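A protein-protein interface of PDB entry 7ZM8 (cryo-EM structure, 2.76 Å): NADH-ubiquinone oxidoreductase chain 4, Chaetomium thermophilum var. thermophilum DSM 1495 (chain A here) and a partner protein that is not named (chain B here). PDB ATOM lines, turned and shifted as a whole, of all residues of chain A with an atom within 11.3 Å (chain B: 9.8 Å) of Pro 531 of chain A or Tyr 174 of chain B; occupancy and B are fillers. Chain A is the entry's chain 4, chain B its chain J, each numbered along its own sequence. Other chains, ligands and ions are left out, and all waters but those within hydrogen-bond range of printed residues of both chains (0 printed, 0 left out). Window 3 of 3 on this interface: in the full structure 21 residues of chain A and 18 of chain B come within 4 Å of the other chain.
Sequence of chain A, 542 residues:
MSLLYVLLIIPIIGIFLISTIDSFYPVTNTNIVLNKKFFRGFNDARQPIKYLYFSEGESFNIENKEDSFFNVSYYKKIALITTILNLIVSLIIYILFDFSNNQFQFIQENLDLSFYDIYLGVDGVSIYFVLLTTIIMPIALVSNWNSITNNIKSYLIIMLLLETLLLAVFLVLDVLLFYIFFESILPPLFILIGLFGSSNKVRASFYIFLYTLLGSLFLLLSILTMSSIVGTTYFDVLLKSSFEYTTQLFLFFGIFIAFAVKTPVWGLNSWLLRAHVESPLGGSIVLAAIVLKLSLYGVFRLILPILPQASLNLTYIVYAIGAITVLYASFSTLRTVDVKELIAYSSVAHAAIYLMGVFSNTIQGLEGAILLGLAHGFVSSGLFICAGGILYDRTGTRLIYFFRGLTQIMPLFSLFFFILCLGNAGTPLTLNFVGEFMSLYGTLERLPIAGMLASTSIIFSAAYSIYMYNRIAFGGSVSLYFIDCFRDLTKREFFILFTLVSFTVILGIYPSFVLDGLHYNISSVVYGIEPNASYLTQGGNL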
ATOM      1  N   GLU A 445     -14.513  -1.662  -6.110  1.00  0.00           N
ATOM      2  CA  GLU A 445     -13.075  -1.639  -5.735  1.00  0.00           C
ATOM      3  C   GLU A 445     -12.244  -2.396  -6.782  1.00  0.00           C
ATOM      4  O   GLU A 445     -11.101  -1.973  -7.026  1.00  0.00           O
ATOM      5  CB  GLU A 445     -12.867  -2.163  -4.312  1.00  0.00           C
ATOM      6  CG  GLU A 445     -11.441  -2.008  -3.817  1.00  0.00           C
ATOM      7  CD  GLU A 445     -11.193  -2.492  -2.402  1.00  0.00           C
ATOM      8  OE1 GLU A 445     -10.275  -1.960  -1.748  1.00  0.00           O
ATOM      9  OE2 GLU A 445     -11.913  -3.404  -1.959  1.00  0.00           O
ATOM     10  N   GLY A 528      -3.402 -12.038  -3.904  1.00  0.00           N
ATOM     11  CA  GLY A 528      -2.700 -10.762  -3.920  1.00  0.00           C
ATOM     12  C   GLY A 528      -1.740 -10.607  -2.783  1.00  0.00           C
ATOM     13  O   GLY A 528      -1.815 -11.375  -1.846  1.00  0.00           O
ATOM     14  N   ILE A 529      -0.855  -9.639  -2.888  1.00  0.00           N
ATOM     15  CA  ILE A 529       0.079  -9.296  -1.825  1.00  0.00           C
ATOM     16  C   ILE A 529       0.048  -7.794  -1.614  1.00  0.00           C
ATOM     17  O   ILE A 529      -0.399  -7.029  -2.469  1.00  0.00           O
ATOM     18  CB  ILE A 529       1.526  -9.746  -2.120  1.00  0.00           C
ATOM     19  CG1 ILE A 529       1.907  -9.424  -3.561  1.00  0.00           C
ATOM     20  CG2 ILE A 529       1.711 -11.223  -1.814  1.00  0.00           C
ATOM     21  CD1 ILE A 529       3.349  -9.667  -3.850  1.00  0.00           C
ATOM     22  N   GLU A 530       0.528  -7.382  -0.451  1.00  0.00           N
ATOM     23  CA  GLU A 530       0.784  -6.003  -0.092  1.00  0.00           C
ATOM     24  C   GLU A 530       2.275  -5.806   0.133  1.00  0.00           C
ATOM     25  O   GLU A 530       2.934  -6.688   0.692  1.00  0.00           O
ATOM     26  CB  GLU A 530       0.007  -5.607   1.166  1.00  0.00           C
ATOM     27  CG  GLU A 530      -1.488  -5.475   0.936  1.00  0.00           C
ATOM     28  CD  GLU A 530      -1.827  -4.320   0.012  1.00  0.00           C
ATOM     29  OE1 GLU A 530      -1.247  -3.228   0.192  1.00  0.00           O
ATOM     30  OE2 GLU A 530      -2.657  -4.508  -0.906  1.00  0.00           O
ATOM     31  N   PRO A 531       2.838  -4.677  -0.300  1.00  0.00           N
ATOM     32  CA  PRO A 531       4.304  -4.573  -0.393  1.00  0.00           C
ATOM     33  C   PRO A 531       5.035  -4.657   0.928  1.00  0.00           C
ATOM     34  O   PRO A 531       6.228  -4.976   0.930  1.00  0.00           O
ATOM     35  CB  PRO A 531       4.515  -3.208  -1.055  1.00  0.00           C
ATOM     36  CG  PRO A 531       3.277  -2.467  -0.796  1.00  0.00           C
ATOM     37  CD  PRO A 531       2.168  -3.456  -0.763  1.00  0.00           C
ATOM     38  N   ASN A 532       4.368  -4.427   2.055  1.00  0.00           N
ATOM     39  CA  ASN A 532       5.106  -4.382   3.339  1.00  0.00           C
ATOM     40  C   ASN A 532       4.580  -5.475   4.257  1.00  0.00           C
ATOM     41  O   ASN A 532       5.137  -5.654   5.346  1.00  0.00           O
ATOM     42  CB  ASN A 532       5.010  -2.992   3.961  1.00  0.00           C
ATOM     43  CG  ASN A 532       5.645  -1.925   3.096  1.00  0.00           C
ATOM     44  OD1 ASN A 532       4.954  -1.112   2.487  1.00  0.00           O
ATOM     45  ND2 ASN A 532       6.965  -1.933   3.017  1.00  0.00           N
ATOM     46  N   ALA A 533       3.538  -6.175   3.818  1.00  0.00           N
ATOM     47  CA  ALA A 533       2.918  -7.217   4.663  1.00  0.00           C
ATOM     48  C   ALA A 533       3.307  -8.598   4.165  1.00  0.00           C
ATOM     49  O   ALA A 533       2.891  -9.582   4.776  1.00  0.00           O
ATOM     50  CB  ALA A 533       1.425  -7.061   4.587  1.00  0.00           C
ATOM     51  N   SER A 534       4.063  -8.666   3.081  1.00  0.00           N
ATOM     52  CA  SER A 534       4.318 -10.004   2.512  1.00  0.00           C
ATOM     53  C   SER A 534       5.752 -10.454   2.672  1.00  0.00           C
ATOM     54  O   SER A 534       6.591  -9.635   3.083  1.00  0.00           O
ATOM     55  CB  SER A 534       3.990  -9.993   1.054  1.00  0.00           C
ATOM     56  OG  SER A 534       4.548  -8.856   0.413  1.00  0.00           O
ATOM     57  N   TYR A 535       5.999 -11.712   2.344  1.00  0.00           N
ATOM     58  CA  TYR A 535       7.362 -12.235   2.320  1.00  0.00           C
ATOM     59  C   TYR A 535       8.134 -11.813   3.569  1.00  0.00           C
ATOM     60  O   TYR A 535       9.133 -11.095   3.516  1.00  0.00           O
ATOM     61  CB  TYR A 535       8.072 -11.804   1.038  1.00  0.00           C
ATOM     62  CG  TYR A 535       7.450 -12.423  -0.183  1.00  0.00           C
ATOM     63  CD1 TYR A 535       7.603 -13.768  -0.446  1.00  0.00           C
ATOM     64  CD2 TYR A 535       6.686 -11.670  -1.054  1.00  0.00           C
ATOM     65  CE1 TYR A 535       7.024 -14.344  -1.544  1.00  0.00           C
ATOM     66  CE2 TYR A 535       6.105 -12.241  -2.154  1.00  0.00           C
ATOM     67  CZ  TYR A 535       6.279 -13.581  -2.393  1.00  0.00           C
ATOM     68  OH  TYR A 535       5.708 -14.167  -3.489  1.00  0.00           O
ATOM     69  N   LEU A 536       7.636 -12.281   4.707  1.00  0.00           N
ATOM     70  CA  LEU A 536       8.180 -11.905   5.998  1.00  0.00           C
ATOM     71  C   LEU A 536       9.362 -12.791   6.371  1.00  0.00           C
ATOM     72  O   LEU A 536       9.418 -13.972   6.021  1.00  0.00           O
ATOM     73  CB  LEU A 536       7.102 -12.006   7.072  1.00  0.00           C
ATOM     74  CG  LEU A 536       5.866 -11.149   6.835  1.00  0.00           C
ATOM     75  CD1 LEU A 536       4.916 -11.268   8.007  1.00  0.00           C
ATOM     76  CD2 LEU A 536       6.284  -9.712   6.625  1.00  0.00           C
ATOM     77  N   THR A 537      10.308 -12.204   7.095  1.00  0.00           N
ATOM     78  CA  THR A 537      11.483 -12.937   7.546  1.00  0.00           C
ATOM     79  C   THR A 537      11.550 -12.973   9.069  1.00  0.00           C
ATOM     80  O   THR A 537      11.337 -14.018   9.684  1.00  0.00           O
ATOM     81  CB  THR A 537      12.778 -12.318   6.999  1.00  0.00           C
ATOM     82  OG1 THR A 537      12.856 -10.944   7.395  1.00  0.00           O
ATOM     83  CG2 THR A 537      12.802 -12.402   5.481  1.00  0.00           C
ATOM     84  N   GLU B 164       1.975  -5.952 -12.075  1.00  0.00           N
ATOM     85  CA  GLU B 164       1.743  -5.344 -10.743  1.00  0.00           C
ATOM     86  C   GLU B 164       0.514  -4.440 -10.811  1.00  0.00           C
ATOM     87  O   GLU B 164       0.236  -3.910 -11.894  1.00  0.00           O
ATOM     88  CB  GLU B 164       2.980  -4.598 -10.260  1.00  0.00           C
ATOM     89  CG  GLU B 164       4.255  -5.390 -10.448  1.00  0.00           C
ATOM     90  CD  GLU B 164       5.514  -4.647 -10.047  1.00  0.00           C
ATOM     91  OE1 GLU B 164       6.612  -5.198 -10.262  1.00  0.00           O
ATOM     92  OE2 GLU B 164       5.391  -3.524  -9.518  1.00  0.00           O
ATOM     93  N   GLY B 165      -0.188  -4.269  -9.691  1.00  0.00           N
ATOM     94  CA  GLY B 165      -1.436  -3.498  -9.672  1.00  0.00           C
ATOM     95  C   GLY B 165      -2.604  -4.438  -9.533  1.00  0.00           C
ATOM     96  O   GLY B 165      -2.368  -5.645  -9.560  1.00  0.00           O
ATOM     97  N   GLY B 167      -4.211  -5.048  -6.925  1.00  0.00           N
ATOM     98  CA  GLY B 167      -4.040  -5.772  -5.651  1.00  0.00           C
ATOM     99  C   GLY B 167      -2.793  -6.608  -5.633  1.00  0.00           C
ATOM    100  O   GLY B 167      -2.598  -7.341  -4.668  1.00  0.00           O
ATOM    101  N   ILE B 168      -2.052  -6.594  -6.732  1.00  0.00           N
ATOM    102  CA  ILE B 168      -0.758  -7.320  -6.782  1.00  0.00           C
ATOM    103  C   ILE B 168       0.298  -6.258  -6.535  1.00  0.00           C
ATOM    104  O   ILE B 168       0.780  -5.670  -7.506  1.00  0.00           O
ATOM    105  CB  ILE B 168      -0.561  -8.029  -8.134  1.00  0.00           C
ATOM    106  CG1 ILE B 168      -1.782  -8.873  -8.507  1.00  0.00           C
ATOM    107  CG2 ILE B 168       0.710  -8.863  -8.122  1.00  0.00           C
ATOM    108  CD1 ILE B 168      -1.983 -10.082  -7.627  1.00  0.00           C
ATOM    109  N   LYS B 169       0.555  -5.965  -5.264  1.00  0.00           N
ATOM    110  CA  LYS B 169       1.551  -4.925  -4.920  1.00  0.00           C
ATOM    111  C   LYS B 169       2.791  -5.644  -4.402  1.00  0.00           C
ATOM    112  O   LYS B 169       2.865  -5.926  -3.203  1.00  0.00           O
ATOM    113  CB  LYS B 169       0.901  -3.894  -3.995  1.00  0.00           C
ATOM    114  CG  LYS B 169      -0.234  -3.116  -4.650  1.00  0.00           C
ATOM    115  CD  LYS B 169      -1.355  -2.758  -3.708  1.00  0.00           C
ATOM    116  CE  LYS B 169      -1.014  -1.611  -2.783  1.00  0.00           C
ATOM    117  NZ  LYS B 169      -0.939  -0.325  -3.513  1.00  0.00           N
ATOM    118  N   PRO B 170       3.776  -5.934  -5.275  1.00  0.00           N
ATOM    119  CA  PRO B 170       4.958  -6.689  -4.881  1.00  0.00           C
ATOM    120  C   PRO B 170       5.869  -5.804  -4.022  1.00  0.00           C
ATOM    121  O   PRO B 170       5.724  -4.609  -4.118  1.00  0.00           O
ATOM    122  CB  PRO B 170       5.571  -7.110  -6.224  1.00  0.00           C
ATOM    123  CG  PRO B 170       4.473  -6.868  -7.220  1.00  0.00           C
ATOM    124  CD  PRO B 170       3.792  -5.625  -6.698  1.00  0.00           C
ATOM    125  N   PRO B 171       6.780  -6.320  -3.156  1.00  0.00           N
ATOM    126  CA  PRO B 171       7.559  -5.393  -2.353  1.00  0.00           C
ATOM    127  C   PRO B 171       8.298  -4.426  -3.278  1.00  0.00           C
ATOM    128  O   PRO B 171       8.962  -4.872  -4.178  1.00  0.00           O
ATOM    129  CB  PRO B 171       8.526  -6.338  -1.658  1.00  0.00           C
ATOM    130  CG  PRO B 171       7.765  -7.640  -1.556  1.00  0.00           C
ATOM    131  CD  PRO B 171       7.017  -7.733  -2.867  1.00  0.00           C
ATOM    132  N   GLY B 172       8.181  -3.126  -3.019  1.00  0.00           N
ATOM    133  CA  GLY B 172       8.815  -2.105  -3.878  1.00  0.00           C
ATOM    134  C   GLY B 172       7.836  -1.456  -4.843  1.00  0.00           C
ATOM    135  O   GLY B 172       8.295  -0.716  -5.715  1.00  0.00           O
ATOM    136  N   TYR B 173       6.538  -1.715  -4.685  1.00  0.00           N
ATOM    137  CA  TYR B 173       5.504  -1.191  -5.611  1.00  0.00           C
ATOM    138  C   TYR B 173       5.406   0.332  -5.497  1.00  0.00           C
ATOM    139  O   TYR B 173       5.237   0.984  -6.535  1.00  0.00           O
ATOM    140  CB  TYR B 173       4.158  -1.879  -5.357  1.00  0.00           C
ATOM    141  CG  TYR B 173       2.980  -1.295  -6.094  1.00  0.00           C
ATOM    142  CD1 TYR B 173       2.668  -1.702  -7.378  1.00  0.00           C
ATOM    143  CD2 TYR B 173       2.169  -0.340  -5.504  1.00  0.00           C
ATOM    144  CE1 TYR B 173       1.594  -1.164  -8.064  1.00  0.00           C
ATOM    145  CE2 TYR B 173       1.091   0.208  -6.174  1.00  0.00           C
ATOM    146  CZ  TYR B 173       0.802  -0.207  -7.459  1.00  0.00           C
ATOM    147  OH  TYR B 173      -0.261   0.321  -8.128  1.00  0.00           O
ATOM    148  N   TYR B 174       5.468   0.872  -4.284  1.00  0.00           N
ATOM    149  CA  TYR B 174       5.272   2.329  -4.080  1.00  0.00           C
ATOM    150  C   TYR B 174       6.394   3.163  -4.712  1.00  0.00           C
ATOM    151  O   TYR B 174       6.089   4.192  -5.335  1.00  0.00           O
ATOM    152  CB  TYR B 174       5.043   2.627  -2.597  1.00  0.00           C
ATOM    153  CG  TYR B 174       3.762   2.072  -2.034  1.00  0.00           C
ATOM    154  CD1 TYR B 174       2.551   2.281  -2.672  1.00  0.00           C
ATOM    155  CD2 TYR B 174       3.755   1.351  -0.855  1.00  0.00           C
ATOM    156  CE1 TYR B 174       1.368   1.777  -2.159  1.00  0.00           C
ATOM    157  CE2 TYR B 174       2.580   0.846  -0.325  1.00  0.00           C
ATOM    158  CZ  TYR B 174       1.383   1.054  -0.981  1.00  0.00           C
ATOM    159  OH  TYR B 174       0.224   0.555  -0.462  1.00  0.00           O
ATOM    160  N   GLU B 175       7.646   2.749  -4.540  1.00  0.00           N
ATOM    161  CA  GLU B 175       8.797   3.480  -5.131  1.00  0.00           C
ATOM    162  C   GLU B 175       8.716   3.420  -6.654  1.00  0.00           C
ATOM    163  O   GLU B 175       9.034   4.420  -7.300  1.00  0.00           O
ATOM    164  CB  GLU B 175      10.113   2.880  -4.636  1.00  0.00           C
ATOM    165  N   ARG B 176       8.355   2.265  -7.196  1.00  0.00           N
ATOM    166  CA  ARG B 176       8.204   2.136  -8.663  1.00  0.00           C
ATOM    167  C   ARG B 176       7.048   3.018  -9.131  1.00  0.00           C
ATOM    168  O   ARG B 176       7.164   3.620 -10.196  1.00  0.00           O
ATOM    169  CB  ARG B 176       8.055   0.669  -9.073  1.00  0.00           C
ATOM    170  CG  ARG B 176       9.287  -0.189  -8.828  1.00  0.00           C
ATOM    171  CD  ARG B 176       9.142  -1.602  -9.366  1.00  0.00           C
ATOM    172  NE  ARG B 176       8.088  -2.389  -8.737  1.00  0.00           N
ATOM    173  CZ  ARG B 176       8.269  -3.219  -7.718  1.00  0.00           C
ATOM    174  NH1 ARG B 176       7.245  -3.885  -7.214  1.00  0.00           N
ATOM    175  NH2 ARG B 176       9.474  -3.382  -7.201  1.00  0.00           N
ATOM    176  N   ARG B 177       5.966   3.067  -8.360  1.00  0.00           N
ATOM    177  CA  ARG B 177       4.762   3.815  -8.785  1.00  0.00           C
ATOM    178  C   ARG B 177       5.130   5.279  -8.791  1.00  0.00           C
ATOM    179  O   ARG B 177       4.695   5.985  -9.701  1.00  0.00           O
ATOM    180  CB  ARG B 177       3.582   3.538  -7.850  1.00  0.00           C
ATOM    181  CG  ARG B 177       2.240   4.033  -8.363  1.00  0.00           C
ATOM    182  CD  ARG B 177       1.143   3.871  -7.335  1.00  0.00           C
ATOM    183  NE  ARG B 177       0.985   5.096  -6.574  1.00  0.00           N
ATOM    184  CZ  ARG B 177      -0.089   5.870  -6.625  1.00  0.00           C
ATOM    185  NH1 ARG B 177      -0.145   6.973  -5.906  1.00  0.00           N
ATOM    186  NH2 ARG B 177      -1.113   5.528  -7.381  1.00  0.00           N
ATOM    187  N   ALA B 178       5.914   5.699  -7.808  1.00  0.00           N
ATOM    188  CA  ALA B 178       6.375   7.081  -7.822  1.00  0.00           C
ATOM    189  C   ALA B 178       7.135   7.384  -9.102  1.00  0.00           C
ATOM    190  O   ALA B 178       6.900   8.406  -9.754  1.00  0.00           O
ATOM    191  CB  ALA B 178       7.251   7.350  -6.603  1.00  0.00           C
ATOM    192  N   GLN B 179       8.052   6.494  -9.482  1.00  0.00           N
ATOM    193  CA  GLN B 179       8.798   6.686 -10.717  1.00  0.00           C
ATOM    194  C   GLN B 179       7.874   6.657 -11.924  1.00  0.00           C
ATOM    195  O   GLN B 179       8.032   7.451 -12.857  1.00  0.00           O
ATOM    196  CB  GLN B 179       9.881   5.617 -10.838  1.00  0.00           C
ATOM    197  CG  GLN B 179      10.766   5.774 -12.058  1.00  0.00           C
ATOM    198  CD  GLN B 179      11.611   7.027 -11.994  1.00  0.00           C
ATOM    199  OE1 GLN B 179      12.146   7.373 -10.943  1.00  0.00           O
ATOM    200  NE2 GLN B 179      11.730   7.718 -13.121  1.00  0.00           N
ATOM    201  N   ARG B 180       6.911   5.738 -11.929  1.00  0.00           N
ATOM    202  CA  ARG B 180       5.964   5.661 -13.034  1.00  0.00           C
ATOM    203  C   ARG B 180       5.109   6.919 -13.115  1.00  0.00           C
ATOM    204  O   ARG B 180       4.924   7.489 -14.194  1.00  0.00           O
ATOM    205  CB  ARG B 180       5.092   4.420 -12.870  1.00  0.00           C
ATOM    206  CG  ARG B 180       4.133   4.167 -14.001  1.00  0.00           C
ATOM    207  CD  ARG B 180       3.579   2.754 -13.928  1.00  0.00           C
ATOM    208  NE  ARG B 180       2.896   2.488 -12.665  1.00  0.00           N
ATOM    209  CZ  ARG B 180       3.421   1.787 -11.667  1.00  0.00           C
ATOM    210  NH1 ARG B 180       2.732   1.591 -10.555  1.00  0.00           N
ATOM    211  NH2 ARG B 180       4.638   1.284 -11.786  1.00  0.00           N
ATOM    212  N   LEU B 181       4.584   7.368 -11.974  1.00  0.00           N
ATOM    213  CA  LEU B 181       3.716   8.538 -11.964  1.00  0.00           C
ATOM    214  C   LEU B 181       4.477   9.806 -12.309  1.00  0.00           C
ATOM    215  O   LEU B 181       3.932  10.691 -12.972  1.00  0.00           O
ATOM    216  CB  LEU B 181       3.047   8.682 -10.600  1.00  0.00           C
ATOM    217  CG  LEU B 181       1.624   8.149 -10.426  1.00  0.00           C
ATOM    218  CD1 LEU B 181       1.552   6.669 -10.741  1.00  0.00           C
ATOM    219  CD2 LEU B 181       1.152   8.414  -9.013  1.00  0.00           C
ATOM    220  N   LYS B 182       5.727   9.916 -11.855  1.00  0.00           N
ATOM    221  CA  LYS B 182       6.536  11.084 -12.186  1.00  0.00           C
ATOM    222  C   LYS B 182       6.787  11.174 -13.684  1.00  0.00           C
ATOM    223  O   LYS B 182       6.727  12.261 -14.269  1.00  0.00           O
ATOM    224  CB  LYS B 182       7.859  11.032 -11.425  1.00  0.00           C
ATOM    225  CG  LYS B 182       8.868  12.080 -11.858  1.00  0.00           C
ATOM    226  CD  LYS B 182       8.405  13.479 -11.494  1.00  0.00           C
ATOM    227  CE  LYS B 182       9.420  14.521 -11.930  1.00  0.00           C
ATOM    228  NZ  LYS B 182      10.707  14.375 -11.197  1.00  0.00           N
ATOM    229  N   ILE B 189       5.234  12.678  -5.961  1.00  0.00           N
ATOM    230  CA  ILE B 189       4.307  12.247  -4.921  1.00  0.00           C
ATOM    231  C   ILE B 189       4.936  12.516  -3.560  1.00  0.00           C
ATOM    232  O   ILE B 189       6.066  12.095  -3.292  1.00  0.00           O
ATOM    233  CB  ILE B 189       3.947  10.764  -5.079  1.00  0.00           C
ATOM    234  CG1 ILE B 189       3.064  10.554  -6.309  1.00  0.00           C
ATOM    235  CG2 ILE B 189       3.263  10.245  -3.827  1.00  0.00           C
ATOM    236  CD1 ILE B 189       1.825  11.414  -6.333  1.00  0.00           C
ATOM    237  N   ASN B 190       4.201  13.213  -2.695  1.00  0.00           N
ATOM    238  CA  ASN B 190       4.685  13.553  -1.357  1.00  0.00           C
ATOM    239  C   ASN B 190       3.478  13.684  -0.447  1.00  0.00           C
ATOM    240  O   ASN B 190       2.954  14.784  -0.236  1.00  0.00           O
ATOM    241  CB  ASN B 190       5.503  14.843  -1.364  1.00  0.00           C
ATOM    242  CG  ASN B 190       6.191  15.110  -0.040  1.00  0.00           C
ATOM    243  OD1 ASN B 190       6.048  14.349   0.916  1.00  0.00           O
ATOM    244  ND2 ASN B 190       6.940  16.204   0.022  1.00  0.00           N
ATOM    245  N   PRO B 191       2.996  12.574   0.105  1.00  0.00           N
ATOM    246  CA  PRO B 191       1.787  12.622   0.932  1.00  0.00           C
ATOM    247  C   PRO B 191       1.980  13.442   2.202  1.00  0.00           C
ATOM    248  O   PRO B 191       3.087  13.562   2.730  1.00  0.00           O
ATOM    249  CB  PRO B 191       1.530  11.149   1.246  1.00  0.00           C
ATOM    250  CG  PRO B 191       2.132  10.424   0.108  1.00  0.00           C
ATOM    251  CD  PRO B 191       3.369  11.193  -0.231  1.00  0.00           C
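The backbone carbonyl oxygen of Gly 167 of chain B sits at hydrogen-bond distance from the backbone NH of Ile 529 of chain A. The backbone carbonyl oxygen (O) of Ile 529 of chain A lies within hydrogen-bond range of the backbone NH (N) of Lys 169 of chain B, at 3.1 Å. The backbone nitrogen (N) of Pro 531 of chain A lies close to the backbone carbonyl oxygen (O) of Lys 169 of chain B (3.2 Å).
Of the 11 printed residues of chain A, 5 touch a printed residue of chain B. Of the 21 printed residues of chain B, 6 touch a printed residue of chain A. Hydrophobic or aromatic side chains of chain B within 4 Å of the printed part of chain A: Ile 168, Pro 171 and Tyr 174. Among the printed residues, no Asp or Glu carboxylate lies within 4 Å of a Lys or Arg side-chain nitrogen of the other chain.
Gly 528 of chain A touches Gly 167 of chain B. CA of Gly 528 of chain A touches CD1 of Ile 168 of chain B, 3.8 Å away. Ile 529 of chain A touches Pro 170 of chain B (CD1 to CA, 3.5 Å). Glu 530 of chain A touches Lys 169 of chain B. CB of Pro 531 of chain A touches O of Pro 170 of chain B (3.6 Å). Pro 531 of chain A touches Pro 171 of chain B. Tyr 174 of chain B touches Pro 531 of chain A (CE2 to CG, 3.4 Å). Pro 171 of chain B touches Ser 534 of chain A (CG to OG, 3.96 Å).
Tyr 174 of chain B touches just one residue of chain A: Pro 531. Glu 530 of chain A touches just one residue of chain B: Lys 169 (3.4 Å). No residue of chain B comes within 4 Å of Asn 532 of chain A. Printed residues of chain A within 4 Å of Lys 169 of chain B: Ile 529 (3.1 Å), Glu 530 (3.4 Å) and Pro 531 (3.2 Å). Of chain A, only Ile 529 and Pro 531 come within 4 Å of Pro 170 of chain B. Pro 171 of chain B touches just these residues of chain A: Pro 531 and Ser 534. Gly 172 of chain B touches none of the printed residues of chain A. No residue of chain A comes within 4 Å of Tyr 173 of chain B. No residue of chain A comes within 4 Å of Glu 175 of chain B. Arg 177 of chain B touches none of the printed residues of chain A. Ala 178 of chain B touches none of the printed residues of chain A. Printed residues of chain B within 4 Å of Ile 529 of chain A: Gly 167, Lys 169 and Pro 170. Of the printed residues of chain B, Gly 528 of chain A touches Gly 167 and Ile 168. Glu 164 of chain B touches none of the printed residues of chain A. Thr 537 of chain A touches none of the printed residues of chain B.
NZ of Lys 169 of chain B is in hydrogen-bond range of OH of Tyr 174 of chain B (3.4 Å). O of Pro 171 of chain B sits at hydrogen-bond distance from NH2 of Arg 176 of chain B (3.4 Å). The side-chain hydroxyl (OG) of Ser 534 of chain A is in hydrogen-bond range of the backbone carbonyl oxygen (O) of Glu 530 of chain A (2.7 Å).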
